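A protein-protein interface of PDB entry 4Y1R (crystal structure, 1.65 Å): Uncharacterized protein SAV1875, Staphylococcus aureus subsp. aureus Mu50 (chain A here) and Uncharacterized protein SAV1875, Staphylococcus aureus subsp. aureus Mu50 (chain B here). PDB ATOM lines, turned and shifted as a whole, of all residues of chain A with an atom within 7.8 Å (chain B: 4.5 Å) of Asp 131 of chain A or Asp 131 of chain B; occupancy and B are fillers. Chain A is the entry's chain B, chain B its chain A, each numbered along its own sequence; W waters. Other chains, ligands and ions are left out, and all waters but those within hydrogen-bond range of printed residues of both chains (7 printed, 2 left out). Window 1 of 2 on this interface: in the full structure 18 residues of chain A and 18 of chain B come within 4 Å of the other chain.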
ATOM      1  N   ASP A  77      -8.638  -1.488 -18.157  1.00  0.00           N
ATOM      2  CA  ASP A  77      -8.727  -2.695 -18.963  1.00  0.00           C
ATOM      3  C   ASP A  77      -9.791  -2.587 -20.062  1.00  0.00           C
ATOM      4  O   ASP A  77      -9.546  -2.937 -21.210  1.00  0.00           O
ATOM      5  CB  ASP A  77      -8.994  -3.912 -18.075  1.00  0.00           C
ATOM      6  CG  ASP A  77      -8.868  -5.221 -18.846  1.00  0.00           C
ATOM      7  OD1 ASP A  77      -7.826  -5.882 -18.748  1.00  0.00           O
ATOM      8  OD2 ASP A  77      -9.863  -5.625 -19.434  1.00  0.00           O
ATOM      9  N   ARG A  80      -8.513  -0.547 -22.876  1.00  0.00           N
ATOM     10  CA  ARG A  80      -7.516  -1.257 -23.673  1.00  0.00           C
ATOM     11  C   ARG A  80      -8.138  -2.282 -24.590  1.00  0.00           C
ATOM     12  O   ARG A  80      -7.463  -2.799 -25.476  1.00  0.00           O
ATOM     13  CB  ARG A  80      -6.490  -1.939 -22.764  1.00  0.00           C
ATOM     14  CG  ARG A  80      -5.655  -0.945 -21.990  1.00  0.00           C
ATOM     15  CD  ARG A  80      -4.696  -1.701 -21.083  1.00  0.00           C
ATOM     16  NE  ARG A  80      -3.467  -2.050 -21.787  1.00  0.00           N
ATOM     17  CZ  ARG A  80      -2.584  -2.933 -21.332  1.00  0.00           C
ATOM     18  NH1 ARG A  80      -2.905  -3.706 -20.299  1.00  0.00           N
ATOM     19  NH2 ARG A  80      -1.420  -3.088 -21.945  1.00  0.00           N
ATOM     20  N   PRO A 108      -2.187   2.940 -14.710  1.00  0.00           N
ATOM     21  CA  PRO A 108      -0.972   2.848 -15.545  1.00  0.00           C
ATOM     22  C   PRO A 108      -1.000   1.803 -16.681  1.00  0.00           C
ATOM     23  O   PRO A 108      -0.178   1.879 -17.609  1.00  0.00           O
ATOM     24  CB  PRO A 108       0.119   2.513 -14.523  1.00  0.00           C
ATOM     25  CG  PRO A 108      -0.373   3.155 -13.264  1.00  0.00           C
ATOM     26  CD  PRO A 108      -1.866   3.003 -13.278  1.00  0.00           C
ATOM     27  N   GLN A 109      -1.931   0.850 -16.648  1.00  0.00           N
ATOM     28  CA  GLN A 109      -2.068  -0.096 -17.769  1.00  0.00           C
ATOM     29  C   GLN A 109      -2.187   0.625 -19.125  1.00  0.00           C
ATOM     30  O   GLN A 109      -1.646   0.163 -20.129  1.00  0.00           O
ATOM     31  CB  GLN A 109      -3.272  -1.039 -17.575  1.00  0.00           C
ATOM     32  CG  GLN A 109      -3.078  -2.029 -16.442  1.00  0.00           C
ATOM     33  CD  GLN A 109      -4.298  -2.919 -16.284  1.00  0.00           C
ATOM     34  OE1 GLN A 109      -5.408  -2.418 -16.134  1.00  0.00           O
ATOM     35  NE2 GLN A 109      -4.117  -4.233 -16.478  1.00  0.00           N
ATOM     36  N   ILE A 110      -2.904   1.747 -19.165  1.00  0.00           N
ATOM     37  CA  ILE A 110      -3.085   2.454 -20.418  1.00  0.00           C
ATOM     38  C   ILE A 110      -1.757   3.029 -20.897  1.00  0.00           C
ATOM     39  O   ILE A 110      -1.480   3.053 -22.111  1.00  0.00           O
ATOM     40  CB  ILE A 110      -4.136   3.575 -20.286  1.00  0.00           C
ATOM     41  CG1 ILE A 110      -5.510   2.993 -20.489  1.00  0.00           C
ATOM     42  CG2 ILE A 110      -3.951   4.620 -21.383  1.00  0.00           C
ATOM     43  CD1 ILE A 110      -5.788   2.692 -21.943  1.00  0.00           C
ATOM     44  N   ILE A 112       1.013   1.621 -20.700  1.00  0.00           N
ATOM     45  CA  ILE A 112       1.748   0.561 -21.368  1.00  0.00           C
ATOM     46  C   ILE A 112       1.549   0.674 -22.876  1.00  0.00           C
ATOM     47  O   ILE A 112       2.490   0.499 -23.653  1.00  0.00           O
ATOM     48  CB  ILE A 112       1.325  -0.831 -20.847  1.00  0.00           C
ATOM     49  CG1 ILE A 112       1.821  -1.001 -19.410  1.00  0.00           C
ATOM     50  CG2 ILE A 112       1.917  -1.926 -21.709  1.00  0.00           C
ATOM     51  CD1 ILE A 112       1.195  -2.196 -18.695  1.00  0.00           C
ATOM     52  N   ASP A 113       0.340   1.031 -23.289  1.00  0.00           N
ATOM     53  CA  ASP A 113       0.015   1.034 -24.706  1.00  0.00           C
ATOM     54  C   ASP A 113       0.636   2.205 -25.452  1.00  0.00           C
ATOM     55  O   ASP A 113       0.558   2.257 -26.673  1.00  0.00           O
ATOM     56  CB  ASP A 113      -1.503   1.068 -24.907  1.00  0.00           C
ATOM     57  CG  ASP A 113      -2.174  -0.201 -24.441  1.00  0.00           C
ATOM     58  OD1 ASP A 113      -1.469  -1.217 -24.287  1.00  0.00           O
ATOM     59  OD2 ASP A 113      -3.408  -0.171 -24.213  1.00  0.00           O
ATOM     60  N   LEU A 117       7.147   3.838 -21.799  1.00  0.00           N
ATOM     61  CA  LEU A 117       7.522   3.652 -20.407  1.00  0.00           C
ATOM     62  C   LEU A 117       8.938   3.162 -20.164  1.00  0.00           C
ATOM     63  O   LEU A 117       9.351   3.076 -19.005  1.00  0.00           O
ATOM     64  CB  LEU A 117       6.568   2.650 -19.742  1.00  0.00           C
ATOM     65  CG  LEU A 117       5.128   3.147 -19.593  1.00  0.00           C
ATOM     66  CD1 LEU A 117       4.291   2.100 -18.862  1.00  0.00           C
ATOM     67  CD2 LEU A 117       5.058   4.469 -18.842  1.00  0.00           C
ATOM     68  N   LEU A 126      -0.580  -3.700  -7.148  1.00  0.00           N
ATOM     69  CA  LEU A 126       0.285  -4.882  -7.263  1.00  0.00           C
ATOM     70  C   LEU A 126      -0.016  -5.676  -8.534  1.00  0.00           C
ATOM     71  O   LEU A 126       0.896  -6.167  -9.198  1.00  0.00           O
ATOM     72  CB  LEU A 126       0.146  -5.792  -6.036  1.00  0.00           C
ATOM     73  CG  LEU A 126       0.903  -7.124  -6.171  1.00  0.00           C
ATOM     74  CD1 LEU A 126       2.400  -6.893  -6.269  1.00  0.00           C
ATOM     75  CD2 LEU A 126       0.562  -8.020  -4.979  1.00  0.00           C
ATOM     76  N   ASN A 127      -1.300  -5.761  -8.867  1.00  0.00           N
ATOM     77  CA  ASN A 127      -1.786  -6.663  -9.915  1.00  0.00           C
ATOM     78  C   ASN A 127      -1.141  -6.362 -11.269  1.00  0.00           C
ATOM     79  O   ASN A 127      -1.163  -7.198 -12.169  1.00  0.00           O
ATOM     80  CB  ASN A 127      -3.324  -6.552 -10.087  1.00  0.00           C
ATOM     81  CG  ASN A 127      -4.091  -6.703  -8.770  1.00  0.00           C
ATOM     82  OD1 ASN A 127      -5.079  -7.445  -8.698  1.00  0.00           O
ATOM     83  ND2 ASN A 127      -3.691  -5.968  -7.759  1.00  0.00           N
ATOM     84  N   VAL A 128      -0.694  -5.128 -11.465  1.00  0.00           N
ATOM     85  CA  VAL A 128      -0.207  -4.728 -12.788  1.00  0.00           C
ATOM     86  C   VAL A 128       1.275  -4.400 -12.816  1.00  0.00           C
ATOM     87  O   VAL A 128       1.800  -3.983 -13.866  1.00  0.00           O
ATOM     88  CB  VAL A 128      -1.017  -3.553 -13.374  1.00  0.00           C
ATOM     89  CG1 VAL A 128      -2.504  -3.832 -13.236  1.00  0.00           C
ATOM     90  CG2 VAL A 128      -0.701  -2.256 -12.668  1.00  0.00           C
ATOM     91  N   ARG A 129       1.958  -4.578 -11.686  1.00  0.00           N
ATOM     92  CA  ARG A 129       3.372  -4.222 -11.631  1.00  0.00           C
ATOM     93  C   ARG A 129       4.288  -5.018 -12.565  1.00  0.00           C
ATOM     94  O   ARG A 129       5.179  -4.443 -13.195  1.00  0.00           O
ATOM     95  CB  ARG A 129       3.889  -4.302 -10.196  1.00  0.00           C
ATOM     96  CG  ARG A 129       3.325  -3.193  -9.346  1.00  0.00           C
ATOM     97  CD  ARG A 129       3.849  -3.277  -7.937  1.00  0.00           C
ATOM     98  NE  ARG A 129       3.043  -2.405  -7.083  1.00  0.00           N
ATOM     99  CZ  ARG A 129       2.939  -2.526  -5.762  1.00  0.00           C
ATOM    100  NH1 ARG A 129       3.736  -3.362  -5.093  1.00  0.00           N
ATOM    101  NH2 ARG A 129       2.019  -1.820  -5.107  1.00  0.00           N
ATOM    102  N   LYS A 130       4.053  -6.319 -12.683  1.00  0.00           N
ATOM    103  CA  LYS A 130       4.848  -7.119 -13.585  1.00  0.00           C
ATOM    104  C   LYS A 130       4.730  -6.619 -15.019  1.00  0.00           C
ATOM    105  O   LYS A 130       5.725  -6.525 -15.734  1.00  0.00           O
ATOM    106  CB  LYS A 130       4.420  -8.577 -13.516  1.00  0.00           C
ATOM    107  CG  LYS A 130       5.239  -9.451 -14.441  1.00  0.00           C
ATOM    108  CD  LYS A 130       6.704  -9.409 -14.036  1.00  0.00           C
ATOM    109  CE  LYS A 130       7.030 -10.525 -13.061  1.00  0.00           C
ATOM    110  NZ  LYS A 130       8.017 -11.443 -13.686  1.00  0.00           N
ATOM    111  N   ASP A 131       3.531  -6.251 -15.429  1.00  0.00           N
ATOM    112  CA  ASP A 131       3.338  -5.789 -16.799  1.00  0.00           C
ATOM    113  C   ASP A 131       4.033  -4.452 -17.026  1.00  0.00           C
ATOM    114  O   ASP A 131       4.620  -4.230 -18.091  1.00  0.00           O
ATOM    115  CB  ASP A 131       1.846  -5.696 -17.125  1.00  0.00           C
ATOM    116  CG  ASP A 131       1.167  -7.071 -17.143  1.00  0.00           C
ATOM    117  OD1 ASP A 131       1.858  -8.099 -17.320  1.00  0.00           O
ATOM    118  OD2 ASP A 131      -0.055  -7.116 -16.882  1.00  0.00           O
ATOM    119  N   LEU A 132       4.054  -3.601 -15.998  1.00  0.00           N
ATOM    120  CA  LEU A 132       4.759  -2.314 -16.131  1.00  0.00           C
ATOM    121  C   LEU A 132       6.266  -2.563 -16.235  1.00  0.00           C
ATOM    122  O   LEU A 132       6.946  -1.921 -17.043  1.00  0.00           O
ATOM    123  CB  LEU A 132       4.432  -1.403 -14.949  1.00  0.00           C
ATOM    124  CG  LEU A 132       3.001  -0.895 -14.961  1.00  0.00           C
ATOM    125  CD1 LEU A 132       2.682  -0.268 -13.613  1.00  0.00           C
ATOM    126  CD2 LEU A 132       2.835   0.131 -16.091  1.00  0.00           C
ATOM    127  N   SER A 133       6.776  -3.521 -15.463  1.00  0.00           N
ATOM    128  CA  SER A 133       8.192  -3.844 -15.533  1.00  0.00           C
ATOM    129  C   SER A 133       8.542  -4.403 -16.908  1.00  0.00           C
ATOM    130  O   SER A 133       9.572  -4.054 -17.488  1.00  0.00           O
ATOM    131  CB  SER A 133       8.594  -4.835 -14.440  1.00  0.00           C
ATOM    132  OG  SER A 133       8.449  -4.251 -13.161  1.00  0.00           O
ATOM    133  N   ASN A 134       7.677  -5.262 -17.442  1.00  0.00           N
ATOM    134  CA  ASN A 134       7.909  -5.841 -18.758  1.00  0.00           C
ATOM    135  C   ASN A 134       7.856  -4.792 -19.873  1.00  0.00           C
ATOM    136  O   ASN A 134       8.487  -4.978 -20.918  1.00  0.00           O
ATOM    137  CB  ASN A 134       6.922  -6.985 -19.027  1.00  0.00           C
ATOM    138  CG  ASN A 134       7.321  -8.290 -18.347  1.00  0.00           C
ATOM    139  OD1 ASN A 134       8.458  -8.481 -17.910  1.00  0.00           O
ATOM    140  ND2 ASN A 134       6.375  -9.201 -18.267  1.00  0.00           N
ATOM    141  N   ALA A 135       7.176  -3.677 -19.605  1.00  0.00           N
ATOM    142  CA  ALA A 135       7.086  -2.542 -20.563  1.00  0.00           C
ATOM    143  C   ALA A 135       8.349  -1.684 -20.448  1.00  0.00           C
ATOM    144  O   ALA A 135       8.473  -0.654 -21.118  1.00  0.00           O
ATOM    145  CB  ALA A 135       5.832  -1.699 -20.265  1.00  0.00           C
ATOM    146  N   GLY A 136       9.223  -2.030 -19.509  1.00  0.00           N
ATOM    147  CA  GLY A 136      10.517  -1.328 -19.379  1.00  0.00           C
ATOM    148  C   GLY A 136      10.533  -0.289 -18.264  1.00  0.00           C
ATOM    149  O   GLY A 136      11.584   0.364 -18.027  1.00  0.00           O
ATOM    150  N   ALA A 137       9.437  -0.167 -17.512  1.00  0.00           N
ATOM    151  CA  ALA A 137       9.408   0.797 -16.412  1.00  0.00           C
ATOM    152  C   ALA A 137      10.240   0.318 -15.223  1.00  0.00           C
ATOM    153  O   ALA A 137      10.447  -0.892 -15.039  1.00  0.00           O
ATOM    154  CB  ALA A 137       7.970   1.068 -15.968  1.00  0.00           C
ATOM    155  N   VAL A 139       9.683  -0.059 -11.607  1.00  0.00           N
ATOM    156  CA  VAL A 139       8.500  -0.070 -10.778  1.00  0.00           C
ATOM    157  C   VAL A 139       8.896  -0.112  -9.322  1.00  0.00           C
ATOM    158  O   VAL A 139       9.774  -0.893  -8.910  1.00  0.00           O
ATOM    159  CB  VAL A 139       7.616  -1.279 -11.115  1.00  0.00           C
ATOM    160  CG1 VAL A 139       6.415  -1.329 -10.191  1.00  0.00           C
ATOM    161  CG2 VAL A 139       7.195  -1.185 -12.572  1.00  0.00           C
ATOM    162  N   ARG B  80      -3.690 -12.258  -9.742  1.00  0.00           N
ATOM    163  CA  ARG B  80      -2.408 -11.554  -9.779  1.00  0.00           C
ATOM    164  C   ARG B  80      -2.224 -10.545  -8.659  1.00  0.00           C
ATOM    165  O   ARG B  80      -1.127  -9.995  -8.491  1.00  0.00           O
ATOM    166  CB  ARG B  80      -2.197 -10.897 -11.154  1.00  0.00           C
ATOM    167  CG  ARG B  80      -2.166 -11.938 -12.272  1.00  0.00           C
ATOM    168  CD  ARG B  80      -1.951 -11.288 -13.625  1.00  0.00           C
ATOM    169  NE  ARG B  80      -0.534 -10.978 -13.862  1.00  0.00           N
ATOM    170  CZ  ARG B  80      -0.113 -10.166 -14.832  1.00  0.00           C
ATOM    171  NH1 ARG B  80      -0.987  -9.448 -15.529  1.00  0.00           N
ATOM    172  NH2 ARG B  80       1.181 -10.086 -15.106  1.00  0.00           N
ATOM    173  N   ILE B 112       1.993 -14.781 -17.754  1.00  0.00           N
ATOM    174  CA  ILE B 112       3.075 -13.782 -17.731  1.00  0.00           C
ATOM    175  C   ILE B 112       3.896 -13.935 -16.445  1.00  0.00           C
ATOM    176  O   ILE B 112       5.132 -13.823 -16.460  1.00  0.00           O
ATOM    177  CB  ILE B 112       2.475 -12.375 -17.802  1.00  0.00           C
ATOM    178  CG1 ILE B 112       1.838 -12.169 -19.170  1.00  0.00           C
ATOM    179  CG2 ILE B 112       3.516 -11.316 -17.466  1.00  0.00           C
ATOM    180  CD1 ILE B 112       0.932 -10.946 -19.246  1.00  0.00           C
ATOM    181  N   VAL B 128      -5.078  -7.710 -23.537  1.00  0.00           N
ATOM    182  CA  VAL B 128      -3.848  -8.173 -22.879  1.00  0.00           C
ATOM    183  C   VAL B 128      -2.700  -8.510 -23.847  1.00  0.00           C
ATOM    184  O   VAL B 128      -1.641  -8.959 -23.427  1.00  0.00           O
ATOM    185  CB  VAL B 128      -4.100  -9.359 -21.919  1.00  0.00           C
ATOM    186  CG1 VAL B 128      -5.229  -9.063 -20.942  1.00  0.00           C
ATOM    187  CG2 VAL B 128      -4.412 -10.610 -22.674  1.00  0.00           C
ATOM    188  N   ARG B 129      -2.952  -8.427 -25.150  1.00  0.00           N
ATOM    189  CA  ARG B 129      -1.955  -8.860 -26.126  1.00  0.00           C
ATOM    190  C   ARG B 129      -0.617  -8.121 -26.024  1.00  0.00           C
ATOM    191  O   ARG B 129       0.443  -8.738 -26.151  1.00  0.00           O
ATOM    192  CB  ARG B 129      -2.520  -8.747 -27.542  1.00  0.00           C
ATOM    193  CG  ARG B 129      -3.518  -9.846 -27.835  1.00  0.00           C
ATOM    194  CD  ARG B 129      -4.001  -9.755 -29.282  1.00  0.00           C
ATOM    195  NE  ARG B 129      -5.235 -10.511 -29.373  1.00  0.00           N
ATOM    196  CZ  ARG B 129      -6.252 -10.236 -30.170  1.00  0.00           C
ATOM    197  NH1 ARG B 129      -6.138  -9.332 -31.157  1.00  0.00           N
ATOM    198  NH2 ARG B 129      -7.357 -10.946 -30.045  1.00  0.00           N
ATOM    199  N   LYS B 130      -0.654  -6.816 -25.774  1.00  0.00           N
ATOM    200  CA  LYS B 130       0.578  -6.056 -25.607  1.00  0.00           C
ATOM    201  C   LYS B 130       1.390  -6.519 -24.380  1.00  0.00           C
ATOM    202  O   LYS B 130       2.628  -6.648 -24.432  1.00  0.00           O
ATOM    203  CB  LYS B 130       0.280  -4.560 -25.530  1.00  0.00           C
ATOM    204  CG  LYS B 130       1.494  -3.722 -25.185  1.00  0.00           C
ATOM    205  CD  LYS B 130       2.412  -3.584 -26.385  1.00  0.00           C
ATOM    206  CE  LYS B 130       1.789  -2.626 -27.394  1.00  0.00           C
ATOM    207  NZ  LYS B 130       2.806  -1.969 -28.236  1.00  0.00           N
ATOM    208  N   ASP B 131       0.679  -6.860 -23.310  1.00  0.00           N
ATOM    209  CA  ASP B 131       1.376  -7.331 -22.131  1.00  0.00           C
ATOM    210  C   ASP B 131       2.000  -8.681 -22.400  1.00  0.00           C
ATOM    211  O   ASP B 131       3.096  -8.958 -21.909  1.00  0.00           O
ATOM    212  CB  ASP B 131       0.432  -7.370 -20.932  1.00  0.00           C
ATOM    213  CG  ASP B 131      -0.103  -5.981 -20.553  1.00  0.00           C
ATOM    214  OD1 ASP B 131       0.563  -4.949 -20.820  1.00  0.00           O
ATOM    215  OD2 ASP B 131      -1.201  -5.913 -19.961  1.00  0.00           O
ATOM    216  N   LEU B 132       1.305  -9.548 -23.128  1.00  0.00           N
ATOM    217  CA  LEU B 132       1.903 -10.832 -23.503  1.00  0.00           C
ATOM    218  C   LEU B 132       3.130 -10.635 -24.369  1.00  0.00           C
ATOM    219  O   LEU B 132       4.126 -11.345 -24.216  1.00  0.00           O
ATOM    220  CB  LEU B 132       0.902 -11.728 -24.249  1.00  0.00           C
ATOM    221  CG  LEU B 132      -0.195 -12.373 -23.434  1.00  0.00           C
ATOM    222  CD1 LEU B 132      -1.031 -13.148 -24.458  1.00  0.00           C
ATOM    223  CD2 LEU B 132       0.375 -13.314 -22.361  1.00  0.00           C
ATOM    224  N   SER B 133       3.037  -9.709 -25.317  1.00  0.00           N
ATOM    225  CA  SER B 133       4.188  -9.463 -26.170  1.00  0.00           C
ATOM    226  C   SER B 133       5.359  -8.892 -25.352  1.00  0.00           C
ATOM    227  O   SER B 133       6.504  -9.288 -25.542  1.00  0.00           O
ATOM    228  CB  SER B 133       3.813  -8.538 -27.314  1.00  0.00           C
ATOM    229  OG  SER B 133       4.926  -8.400 -28.201  1.00  0.00           O
ATOM    230  N   ASN B 134       5.086  -8.031 -24.377  1.00  0.00           N
ATOM    231  CA  ASN B 134       6.174  -7.501 -23.538  1.00  0.00           C
ATOM    232  C   ASN B 134       6.807  -8.550 -22.624  1.00  0.00           C
ATOM    233  O   ASN B 134       7.944  -8.386 -22.162  1.00  0.00           O
ATOM    234  CB  ASN B 134       5.690  -6.316 -22.694  1.00  0.00           C
ATOM    235  CG  ASN B 134       5.421  -5.057 -23.518  1.00  0.00           C
ATOM    236  OD1 ASN B 134       5.979  -4.865 -24.615  1.00  0.00           O
ATOM    237  ND2 ASN B 134       4.708  -4.115 -22.906  1.00  0.00           N
ATOM    238  N   ALA B 135       6.045  -9.614 -22.351  1.00  0.00           N
ATOM    239  CA  ALA B 135       6.536 -10.782 -21.634  1.00  0.00           C
ATOM    240  C   ALA B 135       7.379 -11.717 -22.487  1.00  0.00           C
ATOM    241  O   ALA B 135       7.910 -12.708 -21.980  1.00  0.00           O
ATOM    242  CB  ALA B 135       5.373 -11.550 -21.014  1.00  0.00           C
HETATM  243  O   HOH W   1      -1.354  -4.868 -17.334  1.00  0.00           O
HETATM  244  O   HOH W   2       3.843  -8.193 -19.349  1.00  0.00           O
HETATM  245  O   HOH W   3      -3.169  -8.094 -13.874  1.00  0.00           O
HETATM  246  O   HOH W   4       4.670  -1.201 -23.874  1.00  0.00           O
HETATM  247  O   HOH W   5       3.384  -5.056 -20.493  1.00  0.00           O
HETATM  248  O   HOH W   6      -1.900  -8.101 -18.742  1.00  0.00           O
HETATM  249  O   HOH W   7       6.953 -12.135 -17.619  1.00  0.00           O
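OD2 of Asp 131 of chain B lies within salt-bridge range of NH1 of Arg 80 of chain A (2.8 Å). The guanidinium group (NH1) of Arg 80 of chain B lies within salt-bridge range of the side-chain carboxylate (OD2) of Asp 131 of chain A (2.9 Å). The side-chain carboxylate (OD2) of Asp 131 of chain A sits close to the side-chain carboxylate (OD2) of Asp 131 of chain B (3.5 Å).
The backbone carbonyl oxygen (O) of Gln 109 of chain A is in hydrogen-bond range of the guanidinium group (NE) of Arg 80 of chain A (3.3 Å). The side-chain carboxylate of Asp 113 of chain A is in salt-bridge range of the guanidinium group of Arg 80 of chain A, at 3.0 Å.
Among the printed residues, merely in contact across the chains: Ile 112 of chain A with Lys 130 of chain B (3.9 Å), Ile 112 of chain A with Asp 131 of chain B (3.4 Å), Ile 112 of chain A with Asn 134 of chain B (3.7 Å), Asp 113 of chain A with Lys 130 of chain B (3.97 Å), Asn 127 of chain A with Arg 80 of chain B (3.7 Å), Lys 130 of chain A with Arg 80 of chain B (3.9 Å), Lys 130 of chain A with Ile 112 of chain B (3.9 Å), Asp 131 of chain A with Ile 112 of chain B (3.6 Å), Asn 134 of chain A with Ile 112 of chain B (3.6 Å), Asn 134 of chain A with Asn 134 of chain B (3.6 Å), Asn 134 of chain A with Ala 135 of chain B (3.7 Å) and Ala 135 of chain A with Asn 134 of chain B (3.7 Å).
Leu 117 of chain A touches none of the printed residues of chain B. Of the printed residues of chain B, Lys 130 of chain A touches Arg 80 (3.9 Å) and Ile 112 (3.9 Å). Of chain B, only Arg 80 (2.9 Å), Ile 112 (3.6 Å) and Asp 131 (3.5 Å) come within 4 Å of Asp 131 of chain A. Printed residues of chain B within 4 Å of Ala 135 of chain A: Asn 134 (3.7 Å). Val 139 of chain A touches none of the printed residues of chain B. Of the printed residues of chain A, Ile 112 of chain B touches Lys 130 (3.9 Å), Asp 131 (3.6 Å) and Asn 134 (3.6 Å). Of chain A, only Arg 80, Ile 112 and Asp 131 come within 4 Å of Asp 131 of chain B. Printed residues of chain A within 4 Å of Asn 134 of chain B: Ile 112 (3.7 Å), Asn 134 (3.6 Å) and Ala 135 (3.7 Å).
Of the 21 printed residues of chain A, 8 touch a printed residue of chain B. Of the 10 printed residues of chain B, 6 touch a printed residue of chain A. Printed residues of chain B that touch a printed residue of chain A: Arg 80, Ile 112, Lys 130, Asp 131, Asn 134 and Ala 135. Among the printed residues, Asp or Glu carboxylates within 4 Å of a Lys or Arg side-chain nitrogen of the other chain: Arg 80 of chain A with Asp 131 of chain B (2.8 Å) and Asp 131 of chain A with Arg 80 of chain B (2.9 Å).
Water W6 lies within hydrogen-bond range of OD2 of Asp 131 of chain B (2.6 Å) and OD2 of Asp 131 of chain A (2.8 Å). Water W1 lies within hydrogen-bond range of the side-chain carboxylate of Asp 131 of chain A, the side-chain carboxylate of Asp 131 of chain B and the side-chain amide nitrogen of Gln 109 of chain A. Water W7 lies within hydrogen-bond range of the backbone carbonyl oxygen of Ile 112 of chain B (2.7 Å) and the side-chain amide nitrogen of Asn 134 of chain A (3.1 Å). Water W4 lies within hydrogen-bond range of the backbone carbonyl oxygen (O) of Ile 112 of chain A (2.8 Å) and the side-chain amide nitrogen (ND2) of Asn 134 of chain B (3.1 Å). Water W3 bridges the backbone carbonyl oxygen of Asn 127 of chain A (2.8 Å) and the guanidinium group of Arg 80 of chain B (3.1 Å). Water W5 lies within hydrogen-bond range of the backbone carbonyl oxygen (O) of Asp 131 of chain A (2.8 Å), the side-chain carboxylate (OD1) of Asp 131 of chain B (2.8 Å) and the side-chain amide nitrogen (ND2) of Asn 134 of chain B (2.9 Å).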
